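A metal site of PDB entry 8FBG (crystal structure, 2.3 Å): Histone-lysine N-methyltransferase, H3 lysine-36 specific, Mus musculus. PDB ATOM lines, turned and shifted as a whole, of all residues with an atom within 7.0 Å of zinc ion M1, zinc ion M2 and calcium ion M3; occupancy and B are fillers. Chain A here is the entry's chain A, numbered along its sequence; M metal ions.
Calcium ion M3 is bound by SG of Cys 45 (2.1 Å), SG of Cys 70 (2.4 Å) and SG of Cys 75 (2.6 Å). Calcium ion M3 has three donor atoms within binding distance.
Asn 63 touches calcium ion M3. Within 4 Å of calcium ion M3: Cys 45, Asn 63, Cys 70 and Cys 75. Along chain A the residues within 4 Å of calcium ion M3 span positions 45 to 75.
Four residues have an atom within 4 Å of zinc ion M2: Cys 55, Cys 70, Cys 75 and Cys 81. Along chain A the residues within 4 Å of zinc ion M2 span positions 55 to 81.
Five residues have an atom within 4 Å of zinc ion M1: Cys 45, Cys 47, Cys 55, Cys 61 and Cys 70. The nearest printed residue that does not touch zinc ion M1 is Cys 75 (4.4 Å).
SG of Cys 61 binds zinc ion M1 (2.3 Å). The side-chain sulfur (SG) of Cys 55 binds zinc ion M1 (2.4 Å). SG of Cys 47 is bound to zinc ion M1. Zinc ion M1 is bound by the side-chain sulfur (SG) of Cys 45 (2.5 Å). Zinc ion M1 has four donor atoms within binding distance.
N of Cys 45 lies within hydrogen-bond range of OD1 of Asn 63, 3.0 Å away. N of Asn 83 lies close to SG of Cys 81 (3.4 Å). The side-chain sulfur (SG) of Cys 75 lies close to the backbone NH (N) of Ala 77, at 3.6 Å. The side-chain sulfur (SG) of Cys 61 sits close to the backbone NH (N) of Arg 64 (3.7 Å). O of Asn 83 sits at hydrogen-bond distance from N of Cys 70, at 2.9 Å. The backbone NH of Ala 77 lies within hydrogen-bond range of the backbone carbonyl oxygen of Cys 47. O of Pro 43 is in hydrogen-bond range of ND2 of Asn 63 (2.9 Å). The side-chain amide nitrogen of Asn 63 lies within hydrogen-bond range of the backbone carbonyl oxygen of Glu 69 (3.3 Å).
Zinc ion M2 is bound by SG of Cys 81 (2.3 Å), SG of Cys 75 (2.3 Å), SG of Cys 55 (2.4 Å) and SG of Cys 70 (2.7 Å). Zinc ion M2 has four donor atoms within binding distance.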
ATOM      1  N   PRO A  43      22.716 -26.041  12.072  1.00  0.00           N
ATOM      2  CA  PRO A  43      23.022 -27.144  11.123  1.00  0.00           C
ATOM      3  C   PRO A  43      23.587 -26.645   9.778  1.00  0.00           C
ATOM      4  O   PRO A  43      23.464 -25.459   9.446  1.00  0.00           O
ATOM      5  CB  PRO A  43      21.671 -27.851  10.948  1.00  0.00           C
ATOM      6  CG  PRO A  43      20.647 -26.893  11.390  1.00  0.00           C
ATOM      7  CD  PRO A  43      21.271 -25.956  12.369  1.00  0.00           C
ATOM      8  N   ARG A  44      24.240 -27.532   9.034  1.00  0.00           N
ATOM      9  CA  ARG A  44      24.852 -27.224   7.735  1.00  0.00           C
ATOM     10  C   ARG A  44      24.297 -28.129   6.654  1.00  0.00           C
ATOM     11  O   ARG A  44      24.673 -29.292   6.587  1.00  0.00           O
ATOM     12  CB  ARG A  44      26.394 -27.346   7.806  1.00  0.00           C
ATOM     13  CG  ARG A  44      27.117 -26.873   6.525  1.00  0.00           C
ATOM     14  CD  ARG A  44      27.155 -25.349   6.367  1.00  0.00           C
ATOM     15  NE  ARG A  44      27.823 -24.725   7.519  1.00  0.00           N
ATOM     16  CZ  ARG A  44      29.141 -24.570   7.640  1.00  0.00           C
ATOM     17  NH1 ARG A  44      29.652 -24.021   8.737  1.00  0.00           N
ATOM     18  NH2 ARG A  44      29.952 -24.943   6.664  1.00  0.00           N
ATOM     19  N   CYS A  45      23.437 -27.571   5.775  1.00  0.00           N
ATOM     20  CA  CYS A  45      22.807 -28.303   4.668  1.00  0.00           C
ATOM     21  C   CYS A  45      23.828 -28.658   3.607  1.00  0.00           C
ATOM     22  O   CYS A  45      24.970 -28.221   3.666  1.00  0.00           O
ATOM     23  CB  CYS A  45      21.650 -27.508   4.079  1.00  0.00           C
ATOM     24  SG  CYS A  45      22.153 -26.111   3.029  1.00  0.00           S
ATOM     25  N   ASN A  46      23.395 -29.473   2.639  1.00  0.00           N
ATOM     26  CA  ASN A  46      24.231 -29.930   1.545  1.00  0.00           C
ATOM     27  C   ASN A  46      23.497 -29.722   0.221  1.00  0.00           C
ATOM     28  O   ASN A  46      23.643 -30.507  -0.714  1.00  0.00           O
ATOM     29  CB  ASN A  46      24.665 -31.398   1.763  1.00  0.00           C
ATOM     30  CG  ASN A  46      23.556 -32.437   1.742  1.00  0.00           C
ATOM     31  OD1 ASN A  46      22.363 -32.148   1.822  1.00  0.00           O
ATOM     32  ND2 ASN A  46      23.954 -33.684   1.637  1.00  0.00           N
ATOM     33  N   CYS A  47      22.719 -28.647   0.145  1.00  0.00           N
ATOM     34  CA  CYS A  47      22.032 -28.255  -1.073  1.00  0.00           C
ATOM     35  C   CYS A  47      23.089 -27.686  -2.006  1.00  0.00           C
ATOM     36  O   CYS A  47      24.071 -27.106  -1.540  1.00  0.00           O
ATOM     37  CB  CYS A  47      20.942 -27.235  -0.795  1.00  0.00           C
ATOM     38  SG  CYS A  47      19.646 -27.829   0.324  1.00  0.00           S
ATOM     39  N   LYS A  48      22.910 -27.920  -3.304  1.00  0.00           N
ATOM     40  CA  LYS A  48      23.827 -27.470  -4.312  1.00  0.00           C
ATOM     41  C   LYS A  48      23.226 -26.306  -5.028  1.00  0.00           C
ATOM     42  O   LYS A  48      21.990 -26.211  -5.121  1.00  0.00           O
ATOM     43  CB  LYS A  48      24.120 -28.622  -5.311  1.00  0.00           C
ATOM     44  N   ASP A  51      20.883 -27.300  -7.862  1.00  0.00           N
ATOM     45  CA  ASP A  51      19.559 -27.873  -7.550  1.00  0.00           C
ATOM     46  C   ASP A  51      18.423 -27.030  -8.142  1.00  0.00           C
ATOM     47  O   ASP A  51      18.589 -25.830  -8.323  1.00  0.00           O
ATOM     48  CB  ASP A  51      19.361 -27.996  -6.027  1.00  0.00           C
ATOM     49  CG  ASP A  51      20.176 -29.082  -5.328  1.00  0.00           C
ATOM     50  OD1 ASP A  51      20.647 -30.021  -6.004  1.00  0.00           O
ATOM     51  OD2 ASP A  51      20.312 -29.002  -4.078  1.00  0.00           O
ATOM     52  N   PRO A  54      17.304 -24.533  -4.651  1.00  0.00           N
ATOM     53  CA  PRO A  54      18.253 -24.793  -3.532  1.00  0.00           C
ATOM     54  C   PRO A  54      17.790 -24.184  -2.212  1.00  0.00           C
ATOM     55  O   PRO A  54      17.523 -22.978  -2.117  1.00  0.00           O
ATOM     56  CB  PRO A  54      19.560 -24.176  -4.034  1.00  0.00           C
ATOM     57  CG  PRO A  54      19.427 -24.143  -5.528  1.00  0.00           C
ATOM     58  CD  PRO A  54      17.981 -23.821  -5.758  1.00  0.00           C
ATOM     59  N   CYS A  55      17.590 -25.072  -1.210  1.00  0.00           N
ATOM     60  CA  CYS A  55      17.132 -24.778   0.153  1.00  0.00           C
ATOM     61  C   CYS A  55      15.671 -24.304   0.195  1.00  0.00           C
ATOM     62  O   CYS A  55      15.222 -23.847   1.243  1.00  0.00           O
ATOM     63  CB  CYS A  55      18.063 -23.787   0.845  1.00  0.00           C
ATOM     64  SG  CYS A  55      19.819 -24.143   0.609  1.00  0.00           S
ATOM     65  N   GLY A  56      14.923 -24.511  -0.890  1.00  0.00           N
ATOM     66  CA  GLY A  56      13.521 -24.117  -1.040  1.00  0.00           C
ATOM     67  C   GLY A  56      12.506 -24.985  -0.326  1.00  0.00           C
ATOM     68  O   GLY A  56      12.868 -26.008   0.255  1.00  0.00           O
ATOM     69  N   SER A  59      12.699 -28.756  -0.991  1.00  0.00           N
ATOM     70  CA  SER A  59      14.020 -29.370  -0.942  1.00  0.00           C
ATOM     71  C   SER A  59      14.232 -30.234   0.322  1.00  0.00           C
ATOM     72  O   SER A  59      13.369 -30.297   1.210  1.00  0.00           O
ATOM     73  CB  SER A  59      15.128 -28.319  -1.051  1.00  0.00           C
ATOM     74  OG  SER A  59      15.224 -27.534   0.125  1.00  0.00           O
ATOM     75  N   GLU A  60      15.380 -30.911   0.365  1.00  0.00           N
ATOM     76  CA  GLU A  60      15.806 -31.757   1.464  1.00  0.00           C
ATOM     77  C   GLU A  60      16.735 -30.960   2.395  1.00  0.00           C
ATOM     78  O   GLU A  60      17.532 -31.577   3.112  1.00  0.00           O
ATOM     79  CB  GLU A  60      16.523 -33.000   0.906  1.00  0.00           C
ATOM     80  CG  GLU A  60      15.635 -33.916   0.069  1.00  0.00           C
ATOM     81  CD  GLU A  60      14.872 -34.946   0.869  1.00  0.00           C
ATOM     82  OE1 GLU A  60      13.739 -34.639   1.314  1.00  0.00           O
ATOM     83  OE2 GLU A  60      15.410 -36.065   1.050  1.00  0.00           O
ATOM     84  N   CYS A  61      16.624 -29.596   2.395  1.00  0.00           N
ATOM     85  CA  CYS A  61      17.455 -28.681   3.209  1.00  0.00           C
ATOM     86  C   CYS A  61      17.268 -28.957   4.693  1.00  0.00           C
ATOM     87  O   CYS A  61      16.201 -28.681   5.216  1.00  0.00           O
ATOM     88  CB  CYS A  61      17.158 -27.214   2.886  1.00  0.00           C
ATOM     89  SG  CYS A  61      18.278 -26.030   3.688  1.00  0.00           S
ATOM     90  N   ILE A  62      18.314 -29.462   5.364  1.00  0.00           N
ATOM     91  CA  ILE A  62      18.238 -29.826   6.783  1.00  0.00           C
ATOM     92  C   ILE A  62      17.951 -28.583   7.662  1.00  0.00           C
ATOM     93  O   ILE A  62      17.183 -28.702   8.613  1.00  0.00           O
ATOM     94  CB  ILE A  62      19.450 -30.639   7.278  1.00  0.00           C
ATOM     95  CG1 ILE A  62      19.336 -30.997   8.778  1.00  0.00           C
ATOM     96  CG2 ILE A  62      20.792 -30.018   6.949  1.00  0.00           C
ATOM     97  N   ASN A  63      18.485 -27.409   7.285  1.00  0.00           N
ATOM     98  CA  ASN A  63      18.238 -26.140   7.973  1.00  0.00           C
ATOM     99  C   ASN A  63      16.736 -25.781   7.918  1.00  0.00           C
ATOM    100  O   ASN A  63      16.143 -25.544   8.968  1.00  0.00           O
ATOM    101  CB  ASN A  63      19.104 -25.016   7.357  1.00  0.00           C
ATOM    102  CG  ASN A  63      20.584 -25.111   7.669  1.00  0.00           C
ATOM    103  OD1 ASN A  63      21.300 -25.979   7.173  1.00  0.00           O
ATOM    104  ND2 ASN A  63      21.083 -24.215   8.494  1.00  0.00           N
ATOM    105  N   ARG A  64      16.117 -25.794   6.695  1.00  0.00           N
ATOM    106  CA  ARG A  64      14.698 -25.437   6.526  1.00  0.00           C
ATOM    107  C   ARG A  64      13.783 -26.362   7.330  1.00  0.00           C
ATOM    108  O   ARG A  64      12.892 -25.863   8.011  1.00  0.00           O
ATOM    109  CB  ARG A  64      14.313 -25.415   5.033  1.00  0.00           C
ATOM    110  CG  ARG A  64      12.802 -25.437   4.759  1.00  0.00           C
ATOM    111  CD  ARG A  64      12.496 -25.316   3.280  1.00  0.00           C
ATOM    112  NE  ARG A  64      12.887 -24.017   2.746  1.00  0.00           N
ATOM    113  CZ  ARG A  64      12.113 -22.943   2.778  1.00  0.00           C
ATOM    114  NH1 ARG A  64      10.900 -23.009   3.313  1.00  0.00           N
ATOM    115  NH2 ARG A  64      12.540 -21.782   2.302  1.00  0.00           N
ATOM    116  N   GLU A  69      17.336 -20.835   9.316  1.00  0.00           N
ATOM    117  CA  GLU A  69      17.682 -20.191   8.072  1.00  0.00           C
ATOM    118  C   GLU A  69      19.140 -20.702   7.797  1.00  0.00           C
ATOM    119  O   GLU A  69      19.815 -21.191   8.722  1.00  0.00           O
ATOM    120  CB  GLU A  69      17.746 -18.684   8.307  1.00  0.00           C
ATOM    121  CG  GLU A  69      16.560 -17.875   7.806  1.00  0.00           C
ATOM    122  CD  GLU A  69      16.952 -16.437   7.554  1.00  0.00           C
ATOM    123  OE1 GLU A  69      18.160 -16.131   7.548  1.00  0.00           O
ATOM    124  OE2 GLU A  69      16.029 -15.611   7.341  1.00  0.00           O
ATOM    125  N   CYS A  70      19.621 -20.556   6.550  1.00  0.00           N
ATOM    126  CA  CYS A  70      21.023 -20.876   6.224  1.00  0.00           C
ATOM    127  C   CYS A  70      21.860 -19.623   6.507  1.00  0.00           C
ATOM    128  O   CYS A  70      21.353 -18.499   6.392  1.00  0.00           O
ATOM    129  CB  CYS A  70      21.159 -21.301   4.770  1.00  0.00           C
ATOM    130  SG  CYS A  70      20.307 -22.843   4.340  1.00  0.00           S
ATOM    131  N   HIS A  71      23.152 -19.790   6.852  1.00  0.00           N
ATOM    132  CA  HIS A  71      24.085 -18.673   7.041  1.00  0.00           C
ATOM    133  C   HIS A  71      24.553 -18.320   5.603  1.00  0.00           C
ATOM    134  O   HIS A  71      24.982 -19.233   4.888  1.00  0.00           O
ATOM    135  CB  HIS A  71      25.233 -19.105   7.968  1.00  0.00           C
ATOM    136  CG  HIS A  71      26.368 -18.142   8.117  1.00  0.00           C
ATOM    137  ND1 HIS A  71      26.526 -17.386   9.263  1.00  0.00           N
ATOM    138  CD2 HIS A  71      27.431 -17.918   7.313  1.00  0.00           C
ATOM    139  CE1 HIS A  71      27.631 -16.679   9.088  1.00  0.00           C
ATOM    140  NE2 HIS A  71      28.212 -16.973   7.929  1.00  0.00           N
ATOM    141  N   VAL A  74      28.179 -19.410   4.353  1.00  0.00           N
ATOM    142  CA  VAL A  74      28.594 -20.802   4.412  1.00  0.00           C
ATOM    143  C   VAL A  74      27.610 -21.703   3.656  1.00  0.00           C
ATOM    144  O   VAL A  74      27.956 -22.870   3.465  1.00  0.00           O
ATOM    145  CB  VAL A  74      28.878 -21.375   5.846  1.00  0.00           C
ATOM    146  CG1 VAL A  74      30.039 -20.673   6.516  1.00  0.00           C
ATOM    147  CG2 VAL A  74      27.636 -21.368   6.732  1.00  0.00           C
ATOM    148  N   CYS A  75      26.402 -21.215   3.240  1.00  0.00           N
ATOM    149  CA  CYS A  75      25.490 -22.149   2.531  1.00  0.00           C
ATOM    150  C   CYS A  75      26.077 -22.595   1.190  1.00  0.00           C
ATOM    151  O   CYS A  75      26.399 -21.718   0.369  1.00  0.00           O
ATOM    152  CB  CYS A  75      24.084 -21.601   2.353  1.00  0.00           C
ATOM    153  SG  CYS A  75      22.931 -22.821   1.651  1.00  0.00           S
ATOM    154  N   PRO A  76      26.220 -23.932   0.936  1.00  0.00           N
ATOM    155  CA  PRO A  76      26.846 -24.375  -0.334  1.00  0.00           C
ATOM    156  C   PRO A  76      26.019 -24.042  -1.573  1.00  0.00           C
ATOM    157  O   PRO A  76      26.555 -24.047  -2.679  1.00  0.00           O
ATOM    158  CB  PRO A  76      27.016 -25.901  -0.166  1.00  0.00           C
ATOM    159  CG  PRO A  76      26.631 -26.216   1.225  1.00  0.00           C
ATOM    160  CD  PRO A  76      25.872 -25.089   1.801  1.00  0.00           C
ATOM    161  N   ALA A  77      24.724 -23.727  -1.380  1.00  0.00           N
ATOM    162  CA  ALA A  77      23.823 -23.353  -2.469  1.00  0.00           C
ATOM    163  C   ALA A  77      24.191 -21.940  -2.956  1.00  0.00           C
ATOM    164  O   ALA A  77      23.773 -21.530  -4.047  1.00  0.00           O
ATOM    165  CB  ALA A  77      22.385 -23.373  -1.982  1.00  0.00           C
ATOM    166  N   GLY A  78      24.979 -21.240  -2.149  1.00  0.00           N
ATOM    167  CA  GLY A  78      25.512 -19.915  -2.446  1.00  0.00           C
ATOM    168  C   GLY A  78      24.426 -18.881  -2.648  1.00  0.00           C
ATOM    169  O   GLY A  78      23.377 -18.964  -2.000  1.00  0.00           O
ATOM    170  N   ARG A  80      22.076 -18.422  -4.711  1.00  0.00           N
ATOM    171  CA  ARG A  80      20.694 -18.779  -4.993  1.00  0.00           C
ATOM    172  C   ARG A  80      20.042 -19.647  -3.870  1.00  0.00           C
ATOM    173  O   ARG A  80      19.008 -20.281  -4.116  1.00  0.00           O
ATOM    174  CB  ARG A  80      20.518 -19.418  -6.384  1.00  0.00           C
ATOM    175  CG  ARG A  80      21.258 -20.696  -6.701  1.00  0.00           C
ATOM    176  CD  ARG A  80      21.061 -20.977  -8.194  1.00  0.00           C
ATOM    177  NE  ARG A  80      19.630 -20.991  -8.573  1.00  0.00           N
ATOM    178  CZ  ARG A  80      18.936 -22.073  -8.889  1.00  0.00           C
ATOM    179  NH1 ARG A  80      17.648 -21.979  -9.202  1.00  0.00           N
ATOM    180  NH2 ARG A  80      19.529 -23.260  -8.928  1.00  0.00           N
ATOM    181  N   CYS A  81      20.580 -19.559  -2.633  1.00  0.00           N
ATOM    182  CA  CYS A  81      20.009 -20.147  -1.414  1.00  0.00           C
ATOM    183  C   CYS A  81      18.598 -19.561  -1.270  1.00  0.00           C
ATOM    184  O   CYS A  81      18.433 -18.349  -1.395  1.00  0.00           O
ATOM    185  CB  CYS A  81      20.870 -19.787  -0.203  1.00  0.00           C
ATOM    186  SG  CYS A  81      20.098 -20.134   1.400  1.00  0.00           S
ATOM    187  N   GLN A  82      17.586 -20.406  -1.014  1.00  0.00           N
ATOM    188  CA  GLN A  82      16.208 -19.946  -0.861  1.00  0.00           C
ATOM    189  C   GLN A  82      15.730 -20.105   0.588  1.00  0.00           C
ATOM    190  O   GLN A  82      14.519 -20.199   0.844  1.00  0.00           O
ATOM    191  CB  GLN A  82      15.281 -20.703  -1.842  1.00  0.00           C
ATOM    192  CG  GLN A  82      15.531 -20.386  -3.303  1.00  0.00           C
ATOM    193  CD  GLN A  82      14.626 -21.147  -4.223  1.00  0.00           C
ATOM    194  OE1 GLN A  82      13.524 -21.573  -3.848  1.00  0.00           O
ATOM    195  NE2 GLN A  82      15.067 -21.328  -5.454  1.00  0.00           N
ATOM    196  N   ASN A  83      16.666 -20.119   1.525  1.00  0.00           N
ATOM    197  CA  ASN A  83      16.343 -20.282   2.952  1.00  0.00           C
ATOM    198  C   ASN A  83      16.917 -19.114   3.786  1.00  0.00           C
ATOM    199  O   ASN A  83      17.645 -19.318   4.777  1.00  0.00           O
ATOM    200  CB  ASN A  83      16.805 -21.635   3.459  1.00  0.00           C
ATOM    201  CG  ASN A  83      16.229 -22.051   4.788  1.00  0.00           C
ATOM    202  OD1 ASN A  83      15.129 -21.627   5.173  1.00  0.00           O
ATOM    203  ND2 ASN A  83      16.970 -22.893   5.515  1.00  0.00           N
ATOM    204  N   GLN A  84      16.575 -17.892   3.376  1.00  0.00           N
ATOM    205  CA  GLN A  84      16.991 -16.657   4.061  1.00  0.00           C
ATOM    206  C   GLN A  84      15.806 -15.681   4.097  1.00  0.00           C
ATOM    207  O   GLN A  84      16.021 -14.479   4.087  1.00  0.00           O
ATOM    208  CB  GLN A  84      18.243 -16.030   3.383  1.00  0.00           C
ATOM    209  CG  GLN A  84      19.523 -16.841   3.637  1.00  0.00           C
ATOM    210  CD  GLN A  84      20.683 -16.481   2.751  1.00  0.00           C
ATOM    211  OE1 GLN A  84      20.886 -15.335   2.362  1.00  0.00           O
ATOM    212  NE2 GLN A  84      21.515 -17.481   2.454  1.00  0.00           N
HETATM  213 ZN    ZN M   1      19.915 -26.063   2.012  1.00  0.00          ZN
HETATM  214 ZN    ZN M   2      20.740 -22.263   1.780  1.00  0.00          ZN
HETATM  215 CA    CA M   3      22.313 -24.138   3.822  1.00  0.00          CA
HETATM  216 CA    CA M   4      23.822 -23.783   5.557  1.00  0.00          CA
